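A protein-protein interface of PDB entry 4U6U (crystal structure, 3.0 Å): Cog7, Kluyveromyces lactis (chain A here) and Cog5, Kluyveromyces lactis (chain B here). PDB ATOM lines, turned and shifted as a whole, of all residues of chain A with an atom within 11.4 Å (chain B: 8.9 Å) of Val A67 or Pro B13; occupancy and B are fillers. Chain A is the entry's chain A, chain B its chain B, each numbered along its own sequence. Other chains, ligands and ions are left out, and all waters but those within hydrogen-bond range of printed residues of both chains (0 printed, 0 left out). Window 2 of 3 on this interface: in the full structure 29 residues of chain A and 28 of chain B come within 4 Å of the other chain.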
ATOM      1  N   THR A  58       0.484   6.311 -21.238  1.00  0.00           N
ATOM      2  CA  THR A  58       1.531   5.682 -22.043  1.00  0.00           C
ATOM      3  C   THR A  58       1.281   5.936 -23.511  1.00  0.00           C
ATOM      4  O   THR A  58       2.186   6.313 -24.247  1.00  0.00           O
ATOM      5  CB  THR A  58       1.622   4.191 -21.762  1.00  0.00           C
ATOM      6  OG1 THR A  58       2.023   4.018 -20.393  1.00  0.00           O
ATOM      7  CG2 THR A  58       2.605   3.502 -22.695  1.00  0.00           C
ATOM      8  N   LYS A  59       0.042   5.789 -23.944  1.00  0.00           N
ATOM      9  CA  LYS A  59      -0.271   6.105 -25.320  1.00  0.00           C
ATOM     10  C   LYS A  59       0.013   7.574 -25.635  1.00  0.00           C
ATOM     11  O   LYS A  59       0.565   7.886 -26.691  1.00  0.00           O
ATOM     12  CB  LYS A  59      -1.719   5.765 -25.608  1.00  0.00           C
ATOM     13  CG  LYS A  59      -1.894   4.502 -26.380  1.00  0.00           C
ATOM     14  CD  LYS A  59      -3.259   3.889 -26.139  1.00  0.00           C
ATOM     15  CE  LYS A  59      -3.187   2.767 -25.110  1.00  0.00           C
ATOM     16  NZ  LYS A  59      -4.544   2.230 -24.818  1.00  0.00           N
ATOM     17  N   GLU A  60      -0.339   8.481 -24.720  1.00  0.00           N
ATOM     18  CA  GLU A  60      -0.112   9.913 -24.969  1.00  0.00           C
ATOM     19  C   GLU A  60       1.377  10.168 -25.074  1.00  0.00           C
ATOM     20  O   GLU A  60       1.829  10.901 -25.973  1.00  0.00           O
ATOM     21  CB  GLU A  60      -0.718  10.799 -23.872  1.00  0.00           C
ATOM     22  CG  GLU A  60      -2.232  10.777 -23.809  1.00  0.00           C
ATOM     23  CD  GLU A  60      -2.897  11.716 -24.794  1.00  0.00           C
ATOM     24  OE1 GLU A  60      -3.439  12.747 -24.344  1.00  0.00           O
ATOM     25  OE2 GLU A  60      -2.918  11.419 -26.005  1.00  0.00           O
ATOM     26  N   LEU A  61       2.136   9.503 -24.195  1.00  0.00           N
ATOM     27  CA  LEU A  61       3.600   9.580 -24.192  1.00  0.00           C
ATOM     28  C   LEU A  61       4.190   9.154 -25.532  1.00  0.00           C
ATOM     29  O   LEU A  61       4.942   9.894 -26.157  1.00  0.00           O
ATOM     30  CB  LEU A  61       4.179   8.700 -23.089  1.00  0.00           C
ATOM     31  CG  LEU A  61       5.277   9.300 -22.216  1.00  0.00           C
ATOM     32  CD1 LEU A  61       5.994   8.225 -21.464  1.00  0.00           C
ATOM     33  CD2 LEU A  61       6.250  10.050 -23.057  1.00  0.00           C
ATOM     34  N   GLU A  62       3.840   7.952 -25.967  1.00  0.00           N
ATOM     35  CA  GLU A  62       4.299   7.448 -27.249  1.00  0.00           C
ATOM     36  C   GLU A  62       4.056   8.473 -28.349  1.00  0.00           C
ATOM     37  O   GLU A  62       4.961   8.782 -29.112  1.00  0.00           O
ATOM     38  CB  GLU A  62       3.590   6.122 -27.560  1.00  0.00           C
ATOM     39  CG  GLU A  62       4.034   5.367 -28.806  1.00  0.00           C
ATOM     40  CD  GLU A  62       3.388   3.994 -28.878  1.00  0.00           C
ATOM     41  OE1 GLU A  62       4.072   2.994 -28.549  1.00  0.00           O
ATOM     42  OE2 GLU A  62       2.188   3.920 -29.239  1.00  0.00           O
ATOM     43  N   SER A  63       2.835   9.008 -28.403  1.00  0.00           N
ATOM     44  CA  SER A  63       2.415   9.926 -29.460  1.00  0.00           C
ATOM     45  C   SER A  63       3.226  11.221 -29.380  1.00  0.00           C
ATOM     46  O   SER A  63       3.598  11.795 -30.395  1.00  0.00           O
ATOM     47  CB  SER A  63       0.914  10.196 -29.371  1.00  0.00           C
ATOM     48  OG  SER A  63       0.464  10.999 -30.447  1.00  0.00           O
ATOM     49  N   THR A  64       3.514  11.664 -28.160  1.00  0.00           N
ATOM     50  CA  THR A  64       4.256  12.904 -27.963  1.00  0.00           C
ATOM     51  C   THR A  64       5.715  12.805 -28.433  1.00  0.00           C
ATOM     52  O   THR A  64       6.219  13.649 -29.177  1.00  0.00           O
ATOM     53  CB  THR A  64       4.260  13.285 -26.484  1.00  0.00           C
ATOM     54  OG1 THR A  64       2.933  13.627 -26.094  1.00  0.00           O
ATOM     55  CG2 THR A  64       5.191  14.460 -26.232  1.00  0.00           C
ATOM     56  N   ILE A  65       6.376  11.743 -28.012  1.00  0.00           N
ATOM     57  CA  ILE A  65       7.746  11.494 -28.389  1.00  0.00           C
ATOM     58  C   ILE A  65       7.908  11.396 -29.917  1.00  0.00           C
ATOM     59  O   ILE A  65       8.923  11.833 -30.441  1.00  0.00           O
ATOM     60  CB  ILE A  65       8.250  10.231 -27.691  1.00  0.00           C
ATOM     61  CG1 ILE A  65       8.440  10.523 -26.212  1.00  0.00           C
ATOM     62  CG2 ILE A  65       9.516   9.726 -28.305  1.00  0.00           C
ATOM     63  CD1 ILE A  65       8.965   9.386 -25.443  1.00  0.00           C
ATOM     64  N   GLN A  66       6.913  10.868 -30.640  1.00  0.00           N
ATOM     65  CA  GLN A  66       6.991  10.825 -32.107  1.00  0.00           C
ATOM     66  C   GLN A  66       7.118  12.205 -32.748  1.00  0.00           C
ATOM     67  O   GLN A  66       7.738  12.345 -33.793  1.00  0.00           O
ATOM     68  CB  GLN A  66       5.770  10.160 -32.729  1.00  0.00           C
ATOM     69  CG  GLN A  66       5.548   8.716 -32.385  1.00  0.00           C
ATOM     70  CD  GLN A  66       4.203   8.234 -32.899  1.00  0.00           C
ATOM     71  OE1 GLN A  66       3.450   9.005 -33.497  1.00  0.00           O
ATOM     72  NE2 GLN A  66       3.892   6.961 -32.667  1.00  0.00           N
ATOM     73  N   VAL A  67       6.521  13.219 -32.137  1.00  0.00           N
ATOM     74  CA  VAL A  67       6.543  14.555 -32.721  1.00  0.00           C
ATOM     75  C   VAL A  67       7.912  15.208 -32.529  1.00  0.00           C
ATOM     76  O   VAL A  67       8.294  16.132 -33.263  1.00  0.00           O
ATOM     77  CB  VAL A  67       5.437  15.449 -32.135  1.00  0.00           C
ATOM     78  CG1 VAL A  67       4.218  14.621 -31.840  1.00  0.00           C
ATOM     79  CG2 VAL A  67       5.909  16.149 -30.900  1.00  0.00           C
ATOM     80  N   LEU A  68       8.649  14.718 -31.541  1.00  0.00           N
ATOM     81  CA  LEU A  68      10.012  15.163 -31.332  1.00  0.00           C
ATOM     82  C   LEU A  68      10.876  14.877 -32.557  1.00  0.00           C
ATOM     83  O   LEU A  68      11.833  15.600 -32.841  1.00  0.00           O
ATOM     84  CB  LEU A  68      10.593  14.456 -30.119  1.00  0.00           C
ATOM     85  CG  LEU A  68      10.676  15.239 -28.830  1.00  0.00           C
ATOM     86  CD1 LEU A  68       9.405  16.010 -28.677  1.00  0.00           C
ATOM     87  CD2 LEU A  68      10.855  14.261 -27.680  1.00  0.00           C
ATOM     88  N   GLN A  69      10.504  13.831 -33.293  1.00  0.00           N
ATOM     89  CA  GLN A  69      11.121  13.520 -34.570  1.00  0.00           C
ATOM     90  C   GLN A  69      10.746  14.565 -35.625  1.00  0.00           C
ATOM     91  O   GLN A  69       9.592  14.635 -36.055  1.00  0.00           O
ATOM     92  CB  GLN A  69      10.720  12.114 -35.014  1.00  0.00           C
ATOM     93  CG  GLN A  69      11.375  11.670 -36.303  1.00  0.00           C
ATOM     94  CD  GLN A  69      12.883  11.541 -36.168  1.00  0.00           C
ATOM     95  OE1 GLN A  69      13.635  12.464 -36.504  1.00  0.00           O
ATOM     96  NE2 GLN A  69      13.334  10.401 -35.654  1.00  0.00           N
ATOM     97  N   LYS A  70      11.752  15.360 -36.010  1.00  0.00           N
ATOM     98  CA  LYS A  70      11.671  16.521 -36.918  1.00  0.00           C
ATOM     99  C   LYS A  70      10.281  16.912 -37.442  1.00  0.00           C
ATOM    100  O   LYS A  70       9.776  16.303 -38.391  1.00  0.00           O
ATOM    101  CB  LYS A  70      12.598  16.292 -38.114  1.00  0.00           C
ATOM    102  CG  LYS A  70      12.527  17.387 -39.158  1.00  0.00           C
ATOM    103  CD  LYS A  70      13.857  17.581 -39.869  1.00  0.00           C
ATOM    104  CE  LYS A  70      14.424  16.278 -40.430  1.00  0.00           C
ATOM    105  NZ  LYS A  70      13.905  15.954 -41.788  1.00  0.00           N
ATOM    106  N   PRO A  71       9.663  17.938 -36.818  1.00  0.00           N
ATOM    107  CA  PRO A  71       8.355  18.471 -37.220  1.00  0.00           C
ATOM    108  C   PRO A  71       8.467  19.662 -38.181  1.00  0.00           C
ATOM    109  O   PRO A  71       7.517  20.435 -38.323  1.00  0.00           O
ATOM    110  CB  PRO A  71       7.729  18.902 -35.884  1.00  0.00           C
ATOM    111  CG  PRO A  71       8.902  19.047 -34.905  1.00  0.00           C
ATOM    112  CD  PRO A  71      10.169  18.621 -35.614  1.00  0.00           C
ATOM    113  N   GLN B   8      10.852  28.123 -30.473  1.00  0.00           N
ATOM    114  CA  GLN B   8      10.873  26.784 -29.886  1.00  0.00           C
ATOM    115  C   GLN B   8       9.482  26.228 -29.675  1.00  0.00           C
ATOM    116  O   GLN B   8       8.940  26.274 -28.564  1.00  0.00           O
ATOM    117  CB  GLN B   8      11.576  26.772 -28.542  1.00  0.00           C
ATOM    118  CG  GLN B   8      12.964  27.320 -28.527  1.00  0.00           C
ATOM    119  CD  GLN B   8      13.313  27.860 -27.155  1.00  0.00           C
ATOM    120  OE1 GLN B   8      12.448  28.360 -26.430  1.00  0.00           O
ATOM    121  NE2 GLN B   8      14.570  27.737 -26.776  1.00  0.00           N
ATOM    122  N   ASP B   9       8.889  25.743 -30.755  1.00  0.00           N
ATOM    123  CA  ASP B   9       7.701  24.913 -30.666  1.00  0.00           C
ATOM    124  C   ASP B   9       8.210  23.489 -30.735  1.00  0.00           C
ATOM    125  O   ASP B   9       7.531  22.590 -31.222  1.00  0.00           O
ATOM    126  CB  ASP B   9       6.691  25.242 -31.753  1.00  0.00           C
ATOM    127  CG  ASP B   9       5.923  26.514 -31.442  1.00  0.00           C
ATOM    128  OD1 ASP B   9       5.675  26.753 -30.238  1.00  0.00           O
ATOM    129  OD2 ASP B   9       5.593  27.278 -32.383  1.00  0.00           O
ATOM    130  N   ILE B  10       9.461  23.341 -30.298  1.00  0.00           N
ATOM    131  CA  ILE B  10      10.159  22.068 -30.182  1.00  0.00           C
ATOM    132  C   ILE B  10      10.502  21.831 -28.706  1.00  0.00           C
ATOM    133  O   ILE B  10      10.793  20.704 -28.307  1.00  0.00           O
ATOM    134  CB  ILE B  10      11.439  22.024 -31.029  1.00  0.00           C
ATOM    135  CG1 ILE B  10      12.374  23.178 -30.646  1.00  0.00           C
ATOM    136  CG2 ILE B  10      11.090  22.042 -32.514  1.00  0.00           C
ATOM    137  CD1 ILE B  10      13.672  23.196 -31.416  1.00  0.00           C
ATOM    138  N   LEU B  11      10.466  22.896 -27.899  1.00  0.00           N
ATOM    139  CA  LEU B  11      10.630  22.762 -26.446  1.00  0.00           C
ATOM    140  C   LEU B  11       9.338  22.295 -25.795  1.00  0.00           C
ATOM    141  O   LEU B  11       9.380  21.484 -24.873  1.00  0.00           O
ATOM    142  CB  LEU B  11      11.099  24.055 -25.766  1.00  0.00           C
ATOM    143  CG  LEU B  11      12.548  24.505 -25.974  1.00  0.00           C
ATOM    144  CD1 LEU B  11      12.947  25.509 -24.901  1.00  0.00           C
ATOM    145  CD2 LEU B  11      13.510  23.324 -25.988  1.00  0.00           C
ATOM    146  N   GLU B  12       8.197  22.822 -26.228  1.00  0.00           N
ATOM    147  CA  GLU B  12       6.922  22.375 -25.655  1.00  0.00           C
ATOM    148  C   GLU B  12       6.735  20.845 -25.739  1.00  0.00           C
ATOM    149  O   GLU B  12       6.422  20.207 -24.730  1.00  0.00           O
ATOM    150  CB  GLU B  12       5.756  23.091 -26.331  1.00  0.00           C
ATOM    151  CG  GLU B  12       5.620  24.517 -25.843  1.00  0.00           C
ATOM    152  CD  GLU B  12       4.407  25.232 -26.393  1.00  0.00           C
ATOM    153  OE1 GLU B  12       4.494  26.471 -26.549  1.00  0.00           O
ATOM    154  OE2 GLU B  12       3.380  24.567 -26.667  1.00  0.00           O
ATOM    155  N   PRO B  13       6.987  20.234 -26.910  1.00  0.00           N
ATOM    156  CA  PRO B  13       6.830  18.780 -26.920  1.00  0.00           C
ATOM    157  C   PRO B  13       7.856  18.107 -26.030  1.00  0.00           C
ATOM    158  O   PRO B  13       7.549  17.107 -25.382  1.00  0.00           O
ATOM    159  CB  PRO B  13       7.038  18.414 -28.383  1.00  0.00           C
ATOM    160  CG  PRO B  13       6.746  19.649 -29.126  1.00  0.00           C
ATOM    161  CD  PRO B  13       7.251  20.745 -28.263  1.00  0.00           C
ATOM    162  N   PHE B  14       9.070  18.635 -26.006  1.00  0.00           N
ATOM    163  CA  PHE B  14      10.057  18.081 -25.102  1.00  0.00           C
ATOM    164  C   PHE B  14       9.562  18.246 -23.647  1.00  0.00           C
ATOM    165  O   PHE B  14       9.650  17.304 -22.862  1.00  0.00           O
ATOM    166  CB  PHE B  14      11.438  18.709 -25.339  1.00  0.00           C
ATOM    167  CG  PHE B  14      12.333  18.656 -24.138  1.00  0.00           C
ATOM    168  CD1 PHE B  14      12.850  17.456 -23.688  1.00  0.00           C
ATOM    169  CD2 PHE B  14      12.655  19.819 -23.444  1.00  0.00           C
ATOM    170  CE1 PHE B  14      13.675  17.415 -22.557  1.00  0.00           C
ATOM    171  CE2 PHE B  14      13.478  19.779 -22.316  1.00  0.00           C
ATOM    172  CZ  PHE B  14      13.987  18.571 -21.875  1.00  0.00           C
ATOM    173  N   GLU B  15       9.015  19.408 -23.285  1.00  0.00           N
ATOM    174  CA  GLU B  15       8.447  19.592 -21.933  1.00  0.00           C
ATOM    175  C   GLU B  15       7.250  18.652 -21.672  1.00  0.00           C
ATOM    176  O   GLU B  15       7.187  18.001 -20.627  1.00  0.00           O
ATOM    177  CB  GLU B  15       8.062  21.055 -21.710  1.00  0.00           C
ATOM    178  CG  GLU B  15       9.259  21.924 -21.346  1.00  0.00           C
ATOM    179  CD  GLU B  15       9.021  23.426 -21.521  1.00  0.00           C
ATOM    180  OE1 GLU B  15      10.038  24.166 -21.624  1.00  0.00           O
ATOM    181  OE2 GLU B  15       7.837  23.857 -21.576  1.00  0.00           O
ATOM    182  N   ARG B  16       6.324  18.548 -22.630  1.00  0.00           N
ATOM    183  CA  ARG B  16       5.118  17.742 -22.431  1.00  0.00           C
ATOM    184  C   ARG B  16       5.498  16.293 -22.182  1.00  0.00           C
ATOM    185  O   ARG B  16       4.927  15.614 -21.317  1.00  0.00           O
ATOM    186  CB  ARG B  16       4.188  17.858 -23.637  1.00  0.00           C
ATOM    187  CG  ARG B  16       3.016  16.890 -23.666  1.00  0.00           C
ATOM    188  CD  ARG B  16       1.843  17.335 -22.806  1.00  0.00           C
ATOM    189  NE  ARG B  16       0.778  16.331 -22.796  1.00  0.00           N
ATOM    190  CZ  ARG B  16      -0.288  16.353 -21.996  1.00  0.00           C
ATOM    191  NH1 ARG B  16      -0.471  17.346 -21.115  1.00  0.00           N
ATOM    192  NH2 ARG B  16      -1.178  15.367 -22.086  1.00  0.00           N
ATOM    193  N   ALA B  17       6.511  15.845 -22.907  1.00  0.00           N
ATOM    194  CA  ALA B  17       6.984  14.478 -22.797  1.00  0.00           C
ATOM    195  C   ALA B  17       7.559  14.188 -21.426  1.00  0.00           C
ATOM    196  O   ALA B  17       7.320  13.133 -20.828  1.00  0.00           O
ATOM    197  CB  ALA B  17       8.021  14.211 -23.860  1.00  0.00           C
ATOM    198  N   LEU B  18       8.341  15.135 -20.933  1.00  0.00           N
ATOM    199  CA  LEU B  18       8.975  14.987 -19.646  1.00  0.00           C
ATOM    200  C   LEU B  18       7.934  14.849 -18.566  1.00  0.00           C
ATOM    201  O   LEU B  18       8.085  14.071 -17.622  1.00  0.00           O
ATOM    202  CB  LEU B  18       9.863  16.190 -19.372  1.00  0.00           C
ATOM    203  CG  LEU B  18      11.309  15.840 -19.086  1.00  0.00           C
ATOM    204  CD1 LEU B  18      11.355  14.583 -18.164  1.00  0.00           C
ATOM    205  CD2 LEU B  18      12.008  15.638 -20.391  1.00  0.00           C
ATOM    206  N   LYS B  19       6.887  15.653 -18.716  1.00  0.00           N
ATOM    207  CA  LYS B  19       5.811  15.719 -17.756  1.00  0.00           C
ATOM    208  C   LYS B  19       5.080  14.400 -17.708  1.00  0.00           C
ATOM    209  O   LYS B  19       4.830  13.845 -16.633  1.00  0.00           O
ATOM    210  CB  LYS B  19       4.863  16.842 -18.132  1.00  0.00           C
ATOM    211  CG  LYS B  19       3.603  16.887 -17.314  1.00  0.00           C
ATOM    212  CD  LYS B  19       3.896  17.158 -15.893  1.00  0.00           C
ATOM    213  CE  LYS B  19       2.638  17.421 -15.128  1.00  0.00           C
ATOM    214  NZ  LYS B  19       3.002  17.879 -13.767  1.00  0.00           N
ATOM    215  N   LEU B  20       4.755  13.905 -18.898  1.00  0.00           N
ATOM    216  CA  LEU B  20       4.070  12.641 -19.065  1.00  0.00           C
ATOM    217  C   LEU B  20       4.865  11.503 -18.405  1.00  0.00           C
ATOM    218  O   LEU B  20       4.277  10.640 -17.742  1.00  0.00           O
ATOM    219  CB  LEU B  20       3.838  12.369 -20.559  1.00  0.00           C
ATOM    220  CG  LEU B  20       2.422  12.579 -21.136  1.00  0.00           C
ATOM    221  CD1 LEU B  20       1.557  13.420 -20.237  1.00  0.00           C
ATOM    222  CD2 LEU B  20       2.435  13.167 -22.534  1.00  0.00           C
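The side-chain hydroxyl (OG1) of Thr A64 is in hydrogen-bond range of the backbone carbonyl oxygen (O) of Glu A60.
Among the printed residues, merely in contact across the chains: Leu A68 with Pro B13, Val A67 with Pro B13, Thr A64 with Leu B20, Thr A64 with Pro B13, Thr A64 with Ala B17, Leu A68 with Phe B14, Leu A61 with Leu B20 and Leu A61 with Ala B17.
Thr A58 touches none of the printed residues of chain B. Of the printed residues of chain B, Leu A61 touches Ala B17 (3.95 Å) and Leu B20 (3.8 Å). Val A67 touches one residue of chain B. Printed residues of chain B within 4 Å of Leu A68: Pro B13 (3.4 Å) and Phe B14 (3.8 Å). Lys A70 touches none of the printed residues of chain B. No residue of chain A comes within 4 Å of Glu B12. Of the printed residues of chain A, Pro B13 touches Thr A64, Val A67 and Leu A68. Glu B15 touches none of the printed residues of chain A. Of chain A, only Leu A61 and Thr A64 come within 4 Å of Ala B17. Of the printed residues of chain A, Leu B20 touches Leu A61 (3.8 Å) and Thr A64 (3.6 Å). The nearest residue of chain B that does not touch Val A67 is Phe B14 (6.3 Å). The nearest residue of chain A that does not touch Pro B13 is Ile A65 (6.1 Å).
Hydrophobic or aromatic side chains of chain A that line the printed part of chain B: Leu A61, Val A67 and Leu A68. Of the 13 printed residues of chain B, 4 touch a printed residue of chain A. Hydrophobic or aromatic side chains of chain B that line the printed part of chain A: Pro B13, Ala B17 and Leu B20. Along chain B the printed residues that touch a printed residue of chain A span positions 13 to 20. Among the printed residues, 8 pairs touch across the chains. Among the printed residues, no Asp or Glu carboxylate lies within 4 Å of a Lys or Arg side-chain nitrogen of the other chain.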
